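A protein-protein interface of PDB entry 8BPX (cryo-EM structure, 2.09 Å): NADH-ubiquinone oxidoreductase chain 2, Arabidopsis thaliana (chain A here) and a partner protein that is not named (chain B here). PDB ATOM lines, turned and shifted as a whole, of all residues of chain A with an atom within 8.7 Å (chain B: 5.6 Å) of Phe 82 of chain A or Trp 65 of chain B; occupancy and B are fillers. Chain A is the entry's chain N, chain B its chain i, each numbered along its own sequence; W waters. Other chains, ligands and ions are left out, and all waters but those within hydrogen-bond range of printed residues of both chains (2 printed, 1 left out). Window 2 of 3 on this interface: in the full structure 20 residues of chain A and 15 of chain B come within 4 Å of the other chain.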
ATOM      1  N   MET A  12      -1.283  14.269  -8.278  1.00  0.00           N
ATOM      2  CA  MET A  12       0.026  14.494  -7.668  1.00  0.00           C
ATOM      3  C   MET A  12       0.821  13.199  -7.513  1.00  0.00           C
ATOM      4  O   MET A  12       1.997  13.138  -7.872  1.00  0.00           O
ATOM      5  CB  MET A  12      -0.129  15.174  -6.307  1.00  0.00           C
ATOM      6  CG  MET A  12       1.141  15.175  -5.472  1.00  0.00           C
ATOM      7  SD  MET A  12       2.481  16.122  -6.217  1.00  0.00           S
ATOM      8  CE  MET A  12       2.053  17.775  -5.685  1.00  0.00           C
ATOM      9  N   ASN A  14       0.601  10.444  -9.156  1.00  0.00           N
ATOM     10  CA  ASN A  14       0.992   9.830 -10.421  1.00  0.00           C
ATOM     11  C   ASN A  14       2.253  10.459 -10.999  1.00  0.00           C
ATOM     12  O   ASN A  14       2.958   9.814 -11.782  1.00  0.00           O
ATOM     13  CB  ASN A  14      -0.154   9.917 -11.427  1.00  0.00           C
ATOM     14  CG  ASN A  14      -1.261   8.929 -11.128  1.00  0.00           C
ATOM     15  OD1 ASN A  14      -1.041   7.923 -10.459  1.00  0.00           O
ATOM     16  ND2 ASN A  14      -2.459   9.213 -11.623  1.00  0.00           N
ATOM     17  N   LEU A  15       2.548  11.712 -10.638  1.00  0.00           N
ATOM     18  CA  LEU A  15       3.803  12.323 -11.066  1.00  0.00           C
ATOM     19  C   LEU A  15       5.002  11.490 -10.639  1.00  0.00           C
ATOM     20  O   LEU A  15       5.996  11.413 -11.368  1.00  0.00           O
ATOM     21  CB  LEU A  15       3.934  13.738 -10.503  1.00  0.00           C
ATOM     22  CG  LEU A  15       2.768  14.713 -10.653  1.00  0.00           C
ATOM     23  CD1 LEU A  15       2.983  15.909  -9.744  1.00  0.00           C
ATOM     24  CD2 LEU A  15       2.615  15.151 -12.096  1.00  0.00           C
ATOM     25  N   PHE A  16       4.919  10.845  -9.477  1.00  0.00           N
ATOM     26  CA  PHE A  16       6.041  10.096  -8.930  1.00  0.00           C
ATOM     27  C   PHE A  16       6.214   8.727  -9.575  1.00  0.00           C
ATOM     28  O   PHE A  16       7.112   7.983  -9.170  1.00  0.00           O
ATOM     29  CB  PHE A  16       5.888   9.967  -7.411  1.00  0.00           C
ATOM     30  CG  PHE A  16       6.024  11.278  -6.684  1.00  0.00           C
ATOM     31  CD1 PHE A  16       4.945  12.140  -6.573  1.00  0.00           C
ATOM     32  CD2 PHE A  16       7.239  11.662  -6.135  1.00  0.00           C
ATOM     33  CE1 PHE A  16       5.071  13.355  -5.920  1.00  0.00           C
ATOM     34  CE2 PHE A  16       7.371  12.876  -5.478  1.00  0.00           C
ATOM     35  CZ  PHE A  16       6.288  13.723  -5.371  1.00  0.00           C
ATOM     36  N   ALA A  18       7.438   8.474 -12.382  1.00  0.00           N
ATOM     37  CA  ALA A  18       8.743   8.651 -13.010  1.00  0.00           C
ATOM     38  C   ALA A  18       9.893   8.229 -12.104  1.00  0.00           C
ATOM     39  O   ALA A  18      11.010   8.038 -12.596  1.00  0.00           O
ATOM     40  CB  ALA A  18       8.931  10.112 -13.429  1.00  0.00           C
ATOM     41  N   VAL A  19       9.659   8.090 -10.800  1.00  0.00           N
ATOM     42  CA  VAL A  19      10.728   7.730  -9.874  1.00  0.00           C
ATOM     43  C   VAL A  19      10.343   6.533  -9.012  1.00  0.00           C
ATOM     44  O   VAL A  19      10.875   6.365  -7.910  1.00  0.00           O
ATOM     45  CB  VAL A  19      11.121   8.925  -8.981  1.00  0.00           C
ATOM     46  CG1 VAL A  19      11.945   9.932  -9.765  1.00  0.00           C
ATOM     47  CG2 VAL A  19       9.891   9.575  -8.369  1.00  0.00           C
ATOM     48  N   THR A  77       8.921   8.297 -18.305  1.00  0.00           N
ATOM     49  CA  THR A  77       8.902   9.593 -18.971  1.00  0.00           C
ATOM     50  C   THR A  77       7.679  10.427 -18.615  1.00  0.00           C
ATOM     51  O   THR A  77       7.494  11.505 -19.184  1.00  0.00           O
ATOM     52  CB  THR A  77       8.958   9.407 -20.487  1.00  0.00           C
ATOM     53  OG1 THR A  77       7.861   8.588 -20.902  1.00  0.00           O
ATOM     54  CG2 THR A  77      10.263   8.742 -20.890  1.00  0.00           C
ATOM     55  N   ILE A  78       6.829   9.947 -17.708  1.00  0.00           N
ATOM     56  CA  ILE A  78       5.648  10.707 -17.322  1.00  0.00           C
ATOM     57  C   ILE A  78       6.069  11.992 -16.618  1.00  0.00           C
ATOM     58  O   ILE A  78       7.117  12.058 -15.960  1.00  0.00           O
ATOM     59  CB  ILE A  78       4.722   9.853 -16.435  1.00  0.00           C
ATOM     60  CG1 ILE A  78       3.257  10.131 -16.766  1.00  0.00           C
ATOM     61  CG2 ILE A  78       4.976  10.112 -14.953  1.00  0.00           C
ATOM     62  CD1 ILE A  78       2.286   9.425 -15.841  1.00  0.00           C
ATOM     63  N   ALA A  79       5.254  13.037 -16.788  1.00  0.00           N
ATOM     64  CA  ALA A  79       5.445  14.322 -16.113  1.00  0.00           C
ATOM     65  C   ALA A  79       6.836  14.897 -16.369  1.00  0.00           C
ATOM     66  O   ALA A  79       7.472  15.451 -15.469  1.00  0.00           O
ATOM     67  CB  ALA A  79       5.180  14.196 -14.610  1.00  0.00           C
ATOM     68  N   HIS A  80       7.312  14.774 -17.611  1.00  0.00           N
ATOM     69  CA  HIS A  80       8.687  15.161 -17.914  1.00  0.00           C
ATOM     70  C   HIS A  80       8.916  16.658 -17.738  1.00  0.00           C
ATOM     71  O   HIS A  80      10.021  17.071 -17.377  1.00  0.00           O
ATOM     72  CB  HIS A  80       9.069  14.723 -19.330  1.00  0.00           C
ATOM     73  CG  HIS A  80       8.366  15.477 -20.416  1.00  0.00           C
ATOM     74  ND1 HIS A  80       6.995  15.516 -20.527  1.00  0.00           N
ATOM     75  CD2 HIS A  80       8.848  16.220 -21.440  1.00  0.00           C
ATOM     76  CE1 HIS A  80       6.660  16.249 -21.574  1.00  0.00           C
ATOM     77  NE2 HIS A  80       7.766  16.689 -22.144  1.00  0.00           N
ATOM     78  N   LEU A  81       7.900  17.484 -17.992  1.00  0.00           N
ATOM     79  CA  LEU A  81       8.052  18.916 -17.754  1.00  0.00           C
ATOM     80  C   LEU A  81       8.207  19.218 -16.269  1.00  0.00           C
ATOM     81  O   LEU A  81       9.034  20.050 -15.885  1.00  0.00           O
ATOM     82  CB  LEU A  81       6.863  19.679 -18.334  1.00  0.00           C
ATOM     83  CG  LEU A  81       6.679  19.584 -19.848  1.00  0.00           C
ATOM     84  CD1 LEU A  81       5.549  20.497 -20.306  1.00  0.00           C
ATOM     85  CD2 LEU A  81       7.973  19.911 -20.575  1.00  0.00           C
ATOM     86  N   PHE A  82       7.419  18.551 -15.422  1.00  0.00           N
ATOM     87  CA  PHE A  82       7.518  18.764 -13.982  1.00  0.00           C
ATOM     88  C   PHE A  82       8.883  18.342 -13.453  1.00  0.00           C
ATOM     89  O   PHE A  82       9.453  19.009 -12.581  1.00  0.00           O
ATOM     90  CB  PHE A  82       6.392  18.009 -13.271  1.00  0.00           C
ATOM     91  CG  PHE A  82       6.500  18.006 -11.771  1.00  0.00           C
ATOM     92  CD1 PHE A  82       5.952  19.037 -11.025  1.00  0.00           C
ATOM     93  CD2 PHE A  82       7.123  16.961 -11.107  1.00  0.00           C
ATOM     94  CE1 PHE A  82       6.036  19.035  -9.645  1.00  0.00           C
ATOM     95  CE2 PHE A  82       7.214  16.955  -9.729  1.00  0.00           C
ATOM     96  CZ  PHE A  82       6.669  17.993  -8.997  1.00  0.00           C
ATOM     97  N   TRP A  83       9.427  17.244 -13.970  1.00  0.00           N
ATOM     98  CA  TRP A  83      10.714  16.723 -13.531  1.00  0.00           C
ATOM     99  C   TRP A  83      11.893  17.296 -14.306  1.00  0.00           C
ATOM    100  O   TRP A  83      13.033  16.910 -14.035  1.00  0.00           O
ATOM    101  CB  TRP A  83      10.738  15.197 -13.660  1.00  0.00           C
ATOM    102  CG  TRP A  83       9.792  14.486 -12.756  1.00  0.00           C
ATOM    103  CD1 TRP A  83       8.679  13.792 -13.121  1.00  0.00           C
ATOM    104  CD2 TRP A  83       9.882  14.384 -11.332  1.00  0.00           C
ATOM    105  NE1 TRP A  83       8.065  13.268 -12.013  1.00  0.00           N
ATOM    106  CE2 TRP A  83       8.785  13.613 -10.900  1.00  0.00           C
ATOM    107  CE3 TRP A  83      10.782  14.869 -10.380  1.00  0.00           C
ATOM    108  CZ2 TRP A  83       8.560  13.320  -9.558  1.00  0.00           C
ATOM    109  CZ3 TRP A  83      10.560  14.573  -9.046  1.00  0.00           C
ATOM    110  CH2 TRP A  83       9.458  13.806  -8.648  1.00  0.00           C
ATOM    111  N   ASN A  84      11.650  18.204 -15.255  1.00  0.00           N
ATOM    112  CA  ASN A  84      12.686  18.560 -16.222  1.00  0.00           C
ATOM    113  C   ASN A  84      13.903  19.191 -15.555  1.00  0.00           C
ATOM    114  O   ASN A  84      15.044  18.912 -15.943  1.00  0.00           O
ATOM    115  CB  ASN A  84      12.124  19.505 -17.281  1.00  0.00           C
ATOM    116  CG  ASN A  84      13.204  20.056 -18.187  1.00  0.00           C
ATOM    117  OD1 ASN A  84      13.858  19.310 -18.913  1.00  0.00           O
ATOM    118  ND2 ASN A  84      13.405  21.364 -18.142  1.00  0.00           N
ATOM    119  N   ASN A  85      13.687  20.049 -14.564  1.00  0.00           N
ATOM    120  CA  ASN A  85      14.796  20.724 -13.904  1.00  0.00           C
ATOM    121  C   ASN A  85      15.476  19.857 -12.852  1.00  0.00           C
ATOM    122  O   ASN A  85      16.360  20.349 -12.144  1.00  0.00           O
ATOM    123  CB  ASN A  85      14.317  22.037 -13.279  1.00  0.00           C
ATOM    124  CG  ASN A  85      14.033  23.100 -14.322  1.00  0.00           C
ATOM    125  OD1 ASN A  85      12.968  23.712 -14.333  1.00  0.00           O
ATOM    126  ND2 ASN A  85      14.980  23.302 -15.226  1.00  0.00           N
ATOM    127  N   LEU A  86      15.092  18.589 -12.744  1.00  0.00           N
ATOM    128  CA  LEU A  86      15.688  17.650 -11.802  1.00  0.00           C
ATOM    129  C   LEU A  86      16.428  16.504 -12.472  1.00  0.00           C
ATOM    130  O   LEU A  86      17.500  16.119 -12.005  1.00  0.00           O
ATOM    131  CB  LEU A  86      14.614  17.070 -10.880  1.00  0.00           C
ATOM    132  CG  LEU A  86      14.057  18.031  -9.831  1.00  0.00           C
ATOM    133  CD1 LEU A  86      15.132  19.016  -9.384  1.00  0.00           C
ATOM    134  CD2 LEU A  86      12.820  18.756 -10.340  1.00  0.00           C
ATOM    135  N   PHE A  87      15.880  15.944 -13.545  1.00  0.00           N
ATOM    136  CA  PHE A  87      16.510  14.845 -14.271  1.00  0.00           C
ATOM    137  C   PHE A  87      15.801  14.696 -15.615  1.00  0.00           C
ATOM    138  O   PHE A  87      14.824  15.392 -15.905  1.00  0.00           O
ATOM    139  CB  PHE A  87      16.475  13.545 -13.461  1.00  0.00           C
ATOM    140  CG  PHE A  87      15.103  13.151 -13.003  1.00  0.00           C
ATOM    141  CD1 PHE A  87      14.196  12.576 -13.881  1.00  0.00           C
ATOM    142  CD2 PHE A  87      14.719  13.350 -11.688  1.00  0.00           C
ATOM    143  CE1 PHE A  87      12.934  12.214 -13.455  1.00  0.00           C
ATOM    144  CE2 PHE A  87      13.459  12.986 -11.257  1.00  0.00           C
ATOM    145  CZ  PHE A  87      12.566  12.421 -12.142  1.00  0.00           C
ATOM    146  N   ASN B  60      13.010  21.358 -25.985  1.00  0.00           N
ATOM    147  CA  ASN B  60      12.354  22.629 -25.702  1.00  0.00           C
ATOM    148  C   ASN B  60      11.513  22.545 -24.432  1.00  0.00           C
ATOM    149  O   ASN B  60      10.443  23.147 -24.334  1.00  0.00           O
ATOM    150  CB  ASN B  60      11.496  23.073 -26.884  1.00  0.00           C
ATOM    151  CG  ASN B  60      12.325  23.489 -28.085  1.00  0.00           C
ATOM    152  OD1 ASN B  60      13.489  23.870 -27.952  1.00  0.00           O
ATOM    153  ND2 ASN B  60      11.725  23.418 -29.270  1.00  0.00           N
ATOM    154  N   ALA B  61      11.994  21.787 -23.446  1.00  0.00           N
ATOM    155  CA  ALA B  61      11.218  21.579 -22.227  1.00  0.00           C
ATOM    156  C   ALA B  61      10.973  22.890 -21.486  1.00  0.00           C
ATOM    157  O   ALA B  61       9.861  23.135 -21.008  1.00  0.00           O
ATOM    158  CB  ALA B  61      11.927  20.572 -21.321  1.00  0.00           C
ATOM    159  N   GLN B  62      11.993  23.747 -21.386  1.00  0.00           N
ATOM    160  CA  GLN B  62      11.838  24.977 -20.614  1.00  0.00           C
ATOM    161  C   GLN B  62      10.843  25.929 -21.276  1.00  0.00           C
ATOM    162  O   GLN B  62      10.089  26.619 -20.584  1.00  0.00           O
ATOM    163  CB  GLN B  62      13.198  25.654 -20.409  1.00  0.00           C
ATOM    164  CG  GLN B  62      13.116  27.087 -19.887  1.00  0.00           C
ATOM    165  CD  GLN B  62      14.473  27.685 -19.538  1.00  0.00           C
ATOM    166  OE1 GLN B  62      15.472  27.432 -20.208  1.00  0.00           O
ATOM    167  NE2 GLN B  62      14.507  28.492 -18.485  1.00  0.00           N
ATOM    168  N   LEU B  63      10.819  25.966 -22.611  1.00  0.00           N
ATOM    169  CA  LEU B  63       9.868  26.819 -23.319  1.00  0.00           C
ATOM    170  C   LEU B  63       8.420  26.471 -23.004  1.00  0.00           C
ATOM    171  O   LEU B  63       7.546  27.331 -23.146  1.00  0.00           O
ATOM    172  CB  LEU B  63      10.098  26.730 -24.827  1.00  0.00           C
ATOM    173  CG  LEU B  63      11.297  27.482 -25.413  1.00  0.00           C
ATOM    174  CD1 LEU B  63      11.077  27.739 -26.885  1.00  0.00           C
ATOM    175  CD2 LEU B  63      11.545  28.785 -24.680  1.00  0.00           C
ATOM    176  N   ARG B  64       8.139  25.238 -22.584  1.00  0.00           N
ATOM    177  CA  ARG B  64       6.778  24.835 -22.257  1.00  0.00           C
ATOM    178  C   ARG B  64       6.505  24.778 -20.762  1.00  0.00           C
ATOM    179  O   ARG B  64       5.345  24.906 -20.359  1.00  0.00           O
ATOM    180  CB  ARG B  64       6.467  23.468 -22.873  1.00  0.00           C
ATOM    181  CG  ARG B  64       7.018  23.291 -24.271  1.00  0.00           C
ATOM    182  CD  ARG B  64       6.128  22.381 -25.097  1.00  0.00           C
ATOM    183  NE  ARG B  64       6.124  21.010 -24.600  1.00  0.00           N
ATOM    184  CZ  ARG B  64       7.153  20.178 -24.681  1.00  0.00           C
ATOM    185  NH1 ARG B  64       8.301  20.543 -25.228  1.00  0.00           N
ATOM    186  NH2 ARG B  64       7.027  18.944 -24.201  1.00  0.00           N
ATOM    187  N   TRP B  65       7.536  24.589 -19.939  1.00  0.00           N
ATOM    188  CA  TRP B  65       7.341  24.530 -18.495  1.00  0.00           C
ATOM    189  C   TRP B  65       7.292  25.924 -17.885  1.00  0.00           C
ATOM    190  O   TRP B  65       6.369  26.246 -17.135  1.00  0.00           O
ATOM    191  CB  TRP B  65       8.456  23.705 -17.850  1.00  0.00           C
ATOM    192  CG  TRP B  65       8.424  23.712 -16.355  1.00  0.00           C
ATOM    193  CD1 TRP B  65       9.354  24.255 -15.519  1.00  0.00           C
ATOM    194  CD2 TRP B  65       7.421  23.131 -15.515  1.00  0.00           C
ATOM    195  NE1 TRP B  65       8.988  24.060 -14.211  1.00  0.00           N
ATOM    196  CE2 TRP B  65       7.805  23.371 -14.180  1.00  0.00           C
ATOM    197  CE3 TRP B  65       6.230  22.443 -15.761  1.00  0.00           C
ATOM    198  CZ2 TRP B  65       7.042  22.945 -13.098  1.00  0.00           C
ATOM    199  CZ3 TRP B  65       5.475  22.017 -14.682  1.00  0.00           C
ATOM    200  CH2 TRP B  65       5.883  22.270 -13.369  1.00  0.00           C
ATOM    201  N   ASP B  66       8.274  26.761 -18.211  1.00  0.00           N
ATOM    202  CA  ASP B  66       8.385  28.081 -17.595  1.00  0.00           C
ATOM    203  C   ASP B  66       7.127  28.940 -17.713  1.00  0.00           C
ATOM    204  O   ASP B  66       6.815  29.651 -16.742  1.00  0.00           O
ATOM    205  CB  ASP B  66       9.605  28.813 -18.174  1.00  0.00           C
ATOM    206  CG  ASP B  66      10.892  28.482 -17.428  1.00  0.00           C
ATOM    207  OD1 ASP B  66      10.877  27.548 -16.603  1.00  0.00           O
ATOM    208  OD2 ASP B  66      11.914  29.156 -17.664  1.00  0.00           O
ATOM    209  N   PRO B  67       6.385  28.955 -18.830  1.00  0.00           N
ATOM    210  CA  PRO B  67       5.119  29.710 -18.828  1.00  0.00           C
ATOM    211  C   PRO B  67       4.141  29.243 -17.763  1.00  0.00           C
ATOM    212  O   PRO B  67       3.336  30.049 -17.286  1.00  0.00           O
ATOM    213  CB  PRO B  67       4.559  29.491 -20.241  1.00  0.00           C
ATOM    214  CG  PRO B  67       5.713  29.090 -21.075  1.00  0.00           C
ATOM    215  CD  PRO B  67       6.762  28.502 -20.181  1.00  0.00           C
ATOM    216  N   GLN B  68       4.188  27.966 -17.373  1.00  0.00           N
ATOM    217  CA  GLN B  68       3.267  27.462 -16.360  1.00  0.00           C
ATOM    218  C   GLN B  68       3.596  27.976 -14.960  1.00  0.00           C
ATOM    219  O   GLN B  68       2.715  27.974 -14.095  1.00  0.00           O
ATOM    220  CB  GLN B  68       3.262  25.928 -16.365  1.00  0.00           C
ATOM    221  CG  GLN B  68       2.637  25.299 -17.607  1.00  0.00           C
ATOM    222  CD  GLN B  68       2.789  23.785 -17.636  1.00  0.00           C
ATOM    223  OE1 GLN B  68       2.306  23.085 -16.748  1.00  0.00           O
ATOM    224  NE2 GLN B  68       3.473  23.275 -18.653  1.00  0.00           N
ATOM    225  N   ILE B  69       4.834  28.402 -14.713  1.00  0.00           N
ATOM    226  CA  ILE B  69       5.239  28.956 -13.425  1.00  0.00           C
ATOM    227  C   ILE B  69       5.504  30.453 -13.510  1.00  0.00           C
ATOM    228  O   ILE B  69       6.120  31.019 -12.603  1.00  0.00           O
ATOM    229  CB  ILE B  69       6.470  28.227 -12.856  1.00  0.00           C
ATOM    230  CG1 ILE B  69       7.593  28.173 -13.898  1.00  0.00           C
ATOM    231  CG2 ILE B  69       6.087  26.845 -12.335  1.00  0.00           C
ATOM    232  CD1 ILE B  69       8.957  27.856 -13.322  1.00  0.00           C
HETATM  233  O   HOH W   1      10.886  24.471 -12.222  1.00  0.00           O
HETATM  234  O   HOH W   2      12.587  25.271 -17.024  1.00  0.00           O
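Among the printed residues, pairs that only touch across the chains: Asn 84 of chain A with Ala 61 of chain B (3.3 Å), Leu 81 of chain A with Trp 65 of chain B (3.5 Å), Leu 81 of chain A with Ala 61 of chain B (3.8 Å), Leu 81 of chain A with Gln 68 of chain B (3.8 Å), Asn 85 of chain A with Trp 65 of chain B (3.8 Å), Leu 81 of chain A with Arg 64 of chain B (3.9 Å) and Phe 82 of chain A with Trp 65 of chain B (3.9 Å).
Water W1 lies within hydrogen-bond range of the indole nitrogen of Trp 65 of chain B and the side-chain amide oxygen of Asn 85 of chain A. Water W2 lies within hydrogen-bond range of OD1 of Asp 66 of chain B (2.9 Å) and OD1 of Asn 85 of chain A (3.1 Å).
The guanidinium group of Arg 64 of chain B lies close to the backbone carbonyl oxygen of Asn 60 of chain B. The side-chain amide nitrogen (NE2) of Gln 68 of chain B lies within hydrogen-bond range of the backbone carbonyl oxygen (O) of Arg 64 of chain B, 3.0 Å away.
Of the 10 printed residues of chain B, 4 touch a printed residue of chain A. Printed residues of chain B that touch a printed residue of chain A: Ala 61, Arg 64, Trp 65 and Gln 68. Hydrophobic or aromatic side chains of chain A that line the printed part of chain B: His 80, Leu 81 and Phe 82. Along chain A the printed residues that touch a printed residue of chain B span positions 80 to 85.
A ring nitrogen (NE2) of His 80 of chain A lies within hydrogen-bond range of the guanidinium group (NH2) of Arg 64 of chain B.
Trp 65 of chain B touches three residues of chain A. Of the printed residues of chain B, Leu 81 of chain A touches Ala 61 (3.8 Å), Arg 64 (3.9 Å), Trp 65 (3.5 Å) and Gln 68 (3.8 Å). Of the printed residues of chain A, Arg 64 of chain B touches His 80 (3.1 Å) and Leu 81 (3.9 Å). Of the printed residues of chain B, His 80 of chain A touches Arg 64. Of the printed residues of chain B, Asn 84 of chain A touches Ala 61 (3.3 Å).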
